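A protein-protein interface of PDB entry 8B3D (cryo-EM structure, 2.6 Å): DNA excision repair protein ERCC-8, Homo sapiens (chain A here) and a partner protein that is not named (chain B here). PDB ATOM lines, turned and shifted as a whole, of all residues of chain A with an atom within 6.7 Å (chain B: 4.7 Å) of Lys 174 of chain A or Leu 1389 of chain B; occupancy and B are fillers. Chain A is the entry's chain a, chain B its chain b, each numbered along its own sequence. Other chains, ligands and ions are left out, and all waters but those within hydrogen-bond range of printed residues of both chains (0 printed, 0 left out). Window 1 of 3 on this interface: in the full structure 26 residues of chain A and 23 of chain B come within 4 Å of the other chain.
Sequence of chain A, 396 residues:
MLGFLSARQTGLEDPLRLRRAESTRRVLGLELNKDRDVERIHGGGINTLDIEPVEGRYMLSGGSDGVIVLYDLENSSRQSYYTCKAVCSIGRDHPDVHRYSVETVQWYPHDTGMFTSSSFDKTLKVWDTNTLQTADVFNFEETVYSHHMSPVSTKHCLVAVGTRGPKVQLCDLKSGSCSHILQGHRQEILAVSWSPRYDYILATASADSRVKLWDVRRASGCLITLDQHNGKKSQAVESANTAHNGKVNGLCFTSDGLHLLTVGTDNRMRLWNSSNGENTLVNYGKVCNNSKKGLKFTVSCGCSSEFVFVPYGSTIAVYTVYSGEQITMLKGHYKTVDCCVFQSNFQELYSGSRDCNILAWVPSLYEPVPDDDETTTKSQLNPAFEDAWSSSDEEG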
ATOM      1  N   TYR A 108     -27.544  16.601  19.840  1.00  0.00           N
ATOM      2  CA  TYR A 108     -27.800  17.923  20.374  1.00  0.00           C
ATOM      3  C   TYR A 108     -29.107  17.878  21.158  1.00  0.00           C
ATOM      4  O   TYR A 108     -30.123  17.429  20.610  1.00  0.00           O
ATOM      5  CB  TYR A 108     -27.895  18.949  19.250  1.00  0.00           C
ATOM      6  CG  TYR A 108     -28.240  20.341  19.723  1.00  0.00           C
ATOM      7  CD1 TYR A 108     -27.471  20.982  20.680  1.00  0.00           C
ATOM      8  CD2 TYR A 108     -29.338  21.013  19.211  1.00  0.00           C
ATOM      9  CE1 TYR A 108     -27.784  22.252  21.115  1.00  0.00           C
ATOM     10  CE2 TYR A 108     -29.660  22.283  19.639  1.00  0.00           C
ATOM     11  CZ  TYR A 108     -28.880  22.898  20.590  1.00  0.00           C
ATOM     12  OH  TYR A 108     -29.196  24.164  21.020  1.00  0.00           O
ATOM     13  N   MET A 114     -28.929  18.095  14.753  1.00  0.00           N
ATOM     14  CA  MET A 114     -27.492  18.256  14.898  1.00  0.00           C
ATOM     15  C   MET A 114     -27.003  17.256  15.931  1.00  0.00           C
ATOM     16  O   MET A 114     -27.724  16.937  16.878  1.00  0.00           O
ATOM     17  CB  MET A 114     -27.133  19.676  15.344  1.00  0.00           C
ATOM     18  CG  MET A 114     -25.644  19.940  15.462  1.00  0.00           C
ATOM     19  SD  MET A 114     -25.286  21.626  15.969  1.00  0.00           S
ATOM     20  CE  MET A 114     -25.796  21.560  17.683  1.00  0.00           C
ATOM     21  N   VAL A 126     -18.909  18.902  15.005  1.00  0.00           N
ATOM     22  CA  VAL A 126     -20.335  19.169  15.094  1.00  0.00           C
ATOM     23  C   VAL A 126     -20.934  18.940  13.716  1.00  0.00           C
ATOM     24  O   VAL A 126     -20.585  19.646  12.757  1.00  0.00           O
ATOM     25  CB  VAL A 126     -20.604  20.604  15.577  1.00  0.00           C
ATOM     26  CG1 VAL A 126     -22.081  20.900  15.517  1.00  0.00           C
ATOM     27  CG2 VAL A 126     -20.072  20.816  16.988  1.00  0.00           C
ATOM     28  N   ALA A 135     -20.686  20.663  10.374  1.00  0.00           N
ATOM     29  CA  ALA A 135     -20.956  22.080  10.531  1.00  0.00           C
ATOM     30  C   ALA A 135     -19.813  22.816  11.203  1.00  0.00           C
ATOM     31  O   ALA A 135     -19.619  24.007  10.936  1.00  0.00           O
ATOM     32  CB  ALA A 135     -22.230  22.287  11.347  1.00  0.00           C
ATOM     33  N   PHE A 138     -13.695  21.520  16.252  1.00  0.00           N
ATOM     34  CA  PHE A 138     -12.831  22.069  17.284  1.00  0.00           C
ATOM     35  C   PHE A 138     -11.636  21.145  17.450  1.00  0.00           C
ATOM     36  O   PHE A 138     -11.805  19.962  17.755  1.00  0.00           O
ATOM     37  CB  PHE A 138     -13.568  22.207  18.615  1.00  0.00           C
ATOM     38  CG  PHE A 138     -14.734  23.145  18.568  1.00  0.00           C
ATOM     39  CD1 PHE A 138     -15.972  22.709  18.137  1.00  0.00           C
ATOM     40  CD2 PHE A 138     -14.593  24.461  18.967  1.00  0.00           C
ATOM     41  CE1 PHE A 138     -17.045  23.569  18.099  1.00  0.00           C
ATOM     42  CE2 PHE A 138     -15.664  25.324  18.930  1.00  0.00           C
ATOM     43  CZ  PHE A 138     -16.892  24.879  18.497  1.00  0.00           C
ATOM     44  N   MET A 149     -22.621  17.845  26.185  1.00  0.00           N
ATOM     45  CA  MET A 149     -23.432  19.050  26.133  1.00  0.00           C
ATOM     46  C   MET A 149     -24.463  19.009  27.250  1.00  0.00           C
ATOM     47  O   MET A 149     -24.932  17.941  27.648  1.00  0.00           O
ATOM     48  CB  MET A 149     -24.140  19.186  24.788  1.00  0.00           C
ATOM     49  CG  MET A 149     -23.213  19.501  23.649  1.00  0.00           C
ATOM     50  SD  MET A 149     -24.081  20.116  22.203  1.00  0.00           S
ATOM     51  CE  MET A 149     -24.281  18.591  21.293  1.00  0.00           C
ATOM     52  N   LYS A 155     -30.040  28.424  27.644  1.00  0.00           N
ATOM     53  CA  LYS A 155     -29.313  29.687  27.554  1.00  0.00           C
ATOM     54  C   LYS A 155     -27.937  29.501  26.922  1.00  0.00           C
ATOM     55  O   LYS A 155     -27.641  30.108  25.888  1.00  0.00           O
ATOM     56  CB  LYS A 155     -29.190  30.303  28.957  1.00  0.00           C
ATOM     57  N   CYS A 157     -24.800  26.962  25.313  1.00  0.00           N
ATOM     58  CA  CYS A 157     -24.660  25.781  24.471  1.00  0.00           C
ATOM     59  C   CYS A 157     -23.209  25.313  24.486  1.00  0.00           C
ATOM     60  O   CYS A 157     -22.593  25.041  23.455  1.00  0.00           O
ATOM     61  CB  CYS A 157     -25.156  26.078  23.060  1.00  0.00           C
ATOM     62  SG  CYS A 157     -25.177  24.653  21.960  1.00  0.00           S
ATOM     63  N   LEU A 158     -22.646  25.233  25.688  1.00  0.00           N
ATOM     64  CA  LEU A 158     -21.256  24.849  25.869  1.00  0.00           C
ATOM     65  C   LEU A 158     -21.103  23.337  25.818  1.00  0.00           C
ATOM     66  O   LEU A 158     -21.944  22.593  26.329  1.00  0.00           O
ATOM     67  CB  LEU A 158     -20.728  25.366  27.207  1.00  0.00           C
ATOM     68  CG  LEU A 158     -21.045  26.809  27.591  1.00  0.00           C
ATOM     69  CD1 LEU A 158     -20.748  27.037  29.061  1.00  0.00           C
ATOM     70  CD2 LEU A 158     -20.253  27.773  26.728  1.00  0.00           C
ATOM     71  N   CYS A 171     -16.151  24.463  24.963  1.00  0.00           N
ATOM     72  CA  CYS A 171     -16.282  24.942  23.594  1.00  0.00           C
ATOM     73  C   CYS A 171     -17.670  25.528  23.411  1.00  0.00           C
ATOM     74  O   CYS A 171     -18.670  24.825  23.576  1.00  0.00           O
ATOM     75  CB  CYS A 171     -16.048  23.811  22.596  1.00  0.00           C
ATOM     76  SG  CYS A 171     -14.633  22.775  22.982  1.00  0.00           S
ATOM     77  N   ASP A 172     -17.733  26.807  23.070  1.00  0.00           N
ATOM     78  CA  ASP A 172     -19.002  27.480  22.838  1.00  0.00           C
ATOM     79  C   ASP A 172     -19.456  27.186  21.412  1.00  0.00           C
ATOM     80  O   ASP A 172     -18.741  27.502  20.457  1.00  0.00           O
ATOM     81  CB  ASP A 172     -18.851  28.981  23.063  1.00  0.00           C
ATOM     82  CG  ASP A 172     -20.123  29.624  23.548  1.00  0.00           C
ATOM     83  OD1 ASP A 172     -21.187  29.322  22.980  1.00  0.00           O
ATOM     84  OD2 ASP A 172     -20.059  30.436  24.495  1.00  0.00           O
ATOM     85  N   LEU A 173     -20.629  26.567  21.265  1.00  0.00           N
ATOM     86  CA  LEU A 173     -21.161  26.335  19.925  1.00  0.00           C
ATOM     87  C   LEU A 173     -21.752  27.615  19.346  1.00  0.00           C
ATOM     88  O   LEU A 173     -21.632  27.868  18.143  1.00  0.00           O
ATOM     89  CB  LEU A 173     -22.190  25.212  19.952  1.00  0.00           C
ATOM     90  CG  LEU A 173     -21.644  23.807  20.231  1.00  0.00           C
ATOM     91  CD1 LEU A 173     -22.789  22.815  20.361  1.00  0.00           C
ATOM     92  CD2 LEU A 173     -20.661  23.355  19.155  1.00  0.00           C
ATOM     93  N   LYS A 174     -22.389  28.433  20.181  1.00  0.00           N
ATOM     94  CA  LYS A 174     -22.462  29.853  19.877  1.00  0.00           C
ATOM     95  C   LYS A 174     -21.037  30.363  19.711  1.00  0.00           C
ATOM     96  O   LYS A 174     -20.095  29.768  20.238  1.00  0.00           O
ATOM     97  CB  LYS A 174     -23.183  30.613  20.991  1.00  0.00           C
ATOM     98  N   SER A 175     -20.898  31.534  19.073  1.00  0.00           N
ATOM     99  CA  SER A 175     -19.728  31.872  18.254  1.00  0.00           C
ATOM    100  C   SER A 175     -18.436  31.260  18.783  1.00  0.00           C
ATOM    101  O   SER A 175     -18.067  31.473  19.941  1.00  0.00           O
ATOM    102  CB  SER A 175     -19.580  33.392  18.166  1.00  0.00           C
ATOM    103  OG  SER A 175     -18.502  33.753  17.320  1.00  0.00           O
ATOM    104  N   GLY A 176     -17.746  30.504  17.930  1.00  0.00           N
ATOM    105  CA  GLY A 176     -16.895  29.422  18.389  1.00  0.00           C
ATOM    106  C   GLY A 176     -15.744  29.843  19.270  1.00  0.00           C
ATOM    107  O   GLY A 176     -14.736  30.349  18.776  1.00  0.00           O
ATOM    108  N   SER A 177     -15.861  29.582  20.570  1.00  0.00           N
ATOM    109  CA  SER A 177     -14.875  29.997  21.566  1.00  0.00           C
ATOM    110  C   SER A 177     -14.483  28.765  22.372  1.00  0.00           C
ATOM    111  O   SER A 177     -15.182  28.380  23.312  1.00  0.00           O
ATOM    112  CB  SER A 177     -15.432  31.099  22.454  1.00  0.00           C
ATOM    113  OG  SER A 177     -14.485  31.489  23.431  1.00  0.00           O
ATOM    114  N   LEU B1384     -31.723  27.312  21.209  1.00  0.00           N
ATOM    115  CA  LEU B1384     -31.625  27.430  19.761  1.00  0.00           C
ATOM    116  C   LEU B1384     -32.021  26.110  19.112  1.00  0.00           C
ATOM    117  O   LEU B1384     -31.620  25.037  19.570  1.00  0.00           O
ATOM    118  CB  LEU B1384     -30.202  27.812  19.358  1.00  0.00           C
ATOM    119  CG  LEU B1384     -29.640  29.101  19.960  1.00  0.00           C
ATOM    120  CD1 LEU B1384     -28.126  29.031  20.020  1.00  0.00           C
ATOM    121  CD2 LEU B1384     -30.089  30.309  19.160  1.00  0.00           C
ATOM    122  N   SER B1386     -31.129  24.378  16.598  1.00  0.00           N
ATOM    123  CA  SER B1386     -30.113  23.715  15.781  1.00  0.00           C
ATOM    124  C   SER B1386     -30.079  24.190  14.332  1.00  0.00           C
ATOM    125  O   SER B1386     -29.490  23.511  13.488  1.00  0.00           O
ATOM    126  CB  SER B1386     -30.286  22.195  15.805  1.00  0.00           C
ATOM    127  OG  SER B1386     -31.170  21.770  14.785  1.00  0.00           O
ATOM    128  N   SER B1387     -30.691  25.324  14.015  1.00  0.00           N
ATOM    129  CA  SER B1387     -30.675  25.892  12.673  1.00  0.00           C
ATOM    130  C   SER B1387     -30.046  27.270  12.643  1.00  0.00           C
ATOM    131  O   SER B1387     -29.206  27.542  11.784  1.00  0.00           O
ATOM    132  CB  SER B1387     -32.098  25.965  12.111  1.00  0.00           C
ATOM    133  OG  SER B1387     -32.658  24.670  11.990  1.00  0.00           O
ATOM    134  N   SER B1388     -30.431  28.149  13.567  1.00  0.00           N
ATOM    135  CA  SER B1388     -29.667  29.371  13.766  1.00  0.00           C
ATOM    136  C   SER B1388     -28.256  29.040  14.224  1.00  0.00           C
ATOM    137  O   SER B1388     -27.288  29.677  13.796  1.00  0.00           O
ATOM    138  CB  SER B1388     -30.371  30.270  14.782  1.00  0.00           C
ATOM    139  OG  SER B1388     -30.540  29.598  16.017  1.00  0.00           O
ATOM    140  N   LEU B1389     -28.122  28.033  15.086  1.00  0.00           N
ATOM    141  CA  LEU B1389     -26.804  27.618  15.545  1.00  0.00           C
ATOM    142  C   LEU B1389     -26.002  26.996  14.407  1.00  0.00           C
ATOM    143  O   LEU B1389     -24.825  27.324  14.205  1.00  0.00           O
ATOM    144  CB  LEU B1389     -26.956  26.639  16.705  1.00  0.00           C
ATOM    145  CG  LEU B1389     -25.689  26.337  17.501  1.00  0.00           C
ATOM    146  CD1 LEU B1389     -25.456  27.386  18.568  1.00  0.00           C
ATOM    147  CD2 LEU B1389     -25.776  24.955  18.107  1.00  0.00           C
ATOM    148  N   LEU B1390     -26.627  26.095  13.644  1.00  0.00           N
ATOM    149  CA  LEU B1390     -25.947  25.508  12.494  1.00  0.00           C
ATOM    150  C   LEU B1390     -25.630  26.567  11.448  1.00  0.00           C
ATOM    151  O   LEU B1390     -24.562  26.539  10.825  1.00  0.00           O
ATOM    152  CB  LEU B1390     -26.803  24.405  11.869  1.00  0.00           C
ATOM    153  CG  LEU B1390     -26.716  22.981  12.419  1.00  0.00           C
ATOM    154  CD1 LEU B1390     -27.631  22.072  11.622  1.00  0.00           C
ATOM    155  CD2 LEU B1390     -25.304  22.464  12.368  1.00  0.00           C
ATOM    156  N   ALA B1391     -26.558  27.501  11.231  1.00  0.00           N
ATOM    157  CA  ALA B1391     -26.310  28.577  10.278  1.00  0.00           C
ATOM    158  C   ALA B1391     -25.123  29.423  10.712  1.00  0.00           C
ATOM    159  O   ALA B1391     -24.298  29.819   9.882  1.00  0.00           O
ATOM    160  CB  ALA B1391     -27.559  29.443  10.130  1.00  0.00           C
ATOM    161  N   LYS B1392     -25.017  29.713  12.009  1.00  0.00           N
ATOM    162  CA  LYS B1392     -23.887  30.495  12.498  1.00  0.00           C
ATOM    163  C   LYS B1392     -22.582  29.723  12.365  1.00  0.00           C
ATOM    164  O   LYS B1392     -21.540  30.305  12.041  1.00  0.00           O
ATOM    165  CB  LYS B1392     -24.124  30.914  13.945  1.00  0.00           C
ATOM    166  CG  LYS B1392     -25.085  32.080  14.072  1.00  0.00           C
ATOM    167  CD  LYS B1392     -25.344  32.461  15.515  1.00  0.00           C
ATOM    168  CE  LYS B1392     -26.305  33.638  15.599  1.00  0.00           C
ATOM    169  NZ  LYS B1392     -26.502  34.122  16.986  1.00  0.00           N
ATOM    170  N   MET B1393     -22.610  28.413  12.621  1.00  0.00           N
ATOM    171  CA  MET B1393     -21.408  27.612  12.412  1.00  0.00           C
ATOM    172  C   MET B1393     -20.971  27.663  10.954  1.00  0.00           C
ATOM    173  O   MET B1393     -19.783  27.845  10.656  1.00  0.00           O
ATOM    174  CB  MET B1393     -21.637  26.164  12.847  1.00  0.00           C
ATOM    175  CG  MET B1393     -21.749  25.963  14.343  1.00  0.00           C
ATOM    176  SD  MET B1393     -22.060  24.244  14.772  1.00  0.00           S
ATOM    177  CE  MET B1393     -23.141  24.436  16.179  1.00  0.00           C
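The backbone NH (N) of Tyr 108 of chain A lies within hydrogen-bond range of the backbone carbonyl oxygen (O) of Met 114 of chain A (3.0 Å). N of Ala 135 of chain A sits at hydrogen-bond distance from O of Val 126 of chain A (2.6 Å). N of Leu 173 of chain A sits at hydrogen-bond distance from O of Cys 157 of chain A (3.3 Å). N of Lys 174 of chain A sits close to OD1 of Asp 172 of chain A (3.2 Å).
Of the 16 printed residues of chain A, 7 touch a printed residue of chain B. Printed residues of chain B that touch a printed residue of chain A: Leu 1384, Ser 1386, Leu 1389, Leu 1390 and Met 1393. Hydrophobic or aromatic side chains of chain B that line the printed part of chain A: Leu 1389, Leu 1390 and Met 1393. Among the printed residues, no Asp or Glu carboxylate lies within 4 Å of a Lys or Arg side-chain nitrogen of the other chain.
Of chain B, only Leu 1389 comes within 4 Å of Lys 174 of chain A. Ser 177 of chain A touches none of the printed residues of chain B. Of the printed residues of chain A, Leu 1390 of chain B touches Met 114 and Ala 135. Ala 1391 of chain B touches none of the printed residues of chain A. Of the printed residues of chain A, Met 1393 of chain B touches Met 114 (3.5 Å), Val 126 (3.4 Å), Ala 135 (3.5 Å) and Leu 173 (3.97 Å).
Tyr 108 of chain A touches Ser 1386 of chain B. CE of Met 114 of chain A touches CD2 of Leu 1389 of chain B, 3.4 Å away. Met 114 of chain A touches Leu 1390 of chain B. Met 114 of chain A touches Met 1393 of chain B. Ala 135 of chain A touches Leu 1390 of chain B (CB to CD2, 3.2 Å). Ala 135 of chain A touches Met 1393 of chain B (O to CB, 3.5 Å). Leu 1389 of chain B touches Cys 157 of chain A (CD2 to SG, 3.9 Å). Leu 173 of chain A touches Leu 1389 of chain B. Leu 173 of chain A touches Met 1393 of chain B. CD1 of Leu 1389 of chain B touches N of Lys 174 of chain A (3.6 Å).
OH of Tyr 108 of chain A is in hydrogen-bond range of O of Leu 1384 of chain B, at 3.0 Å.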
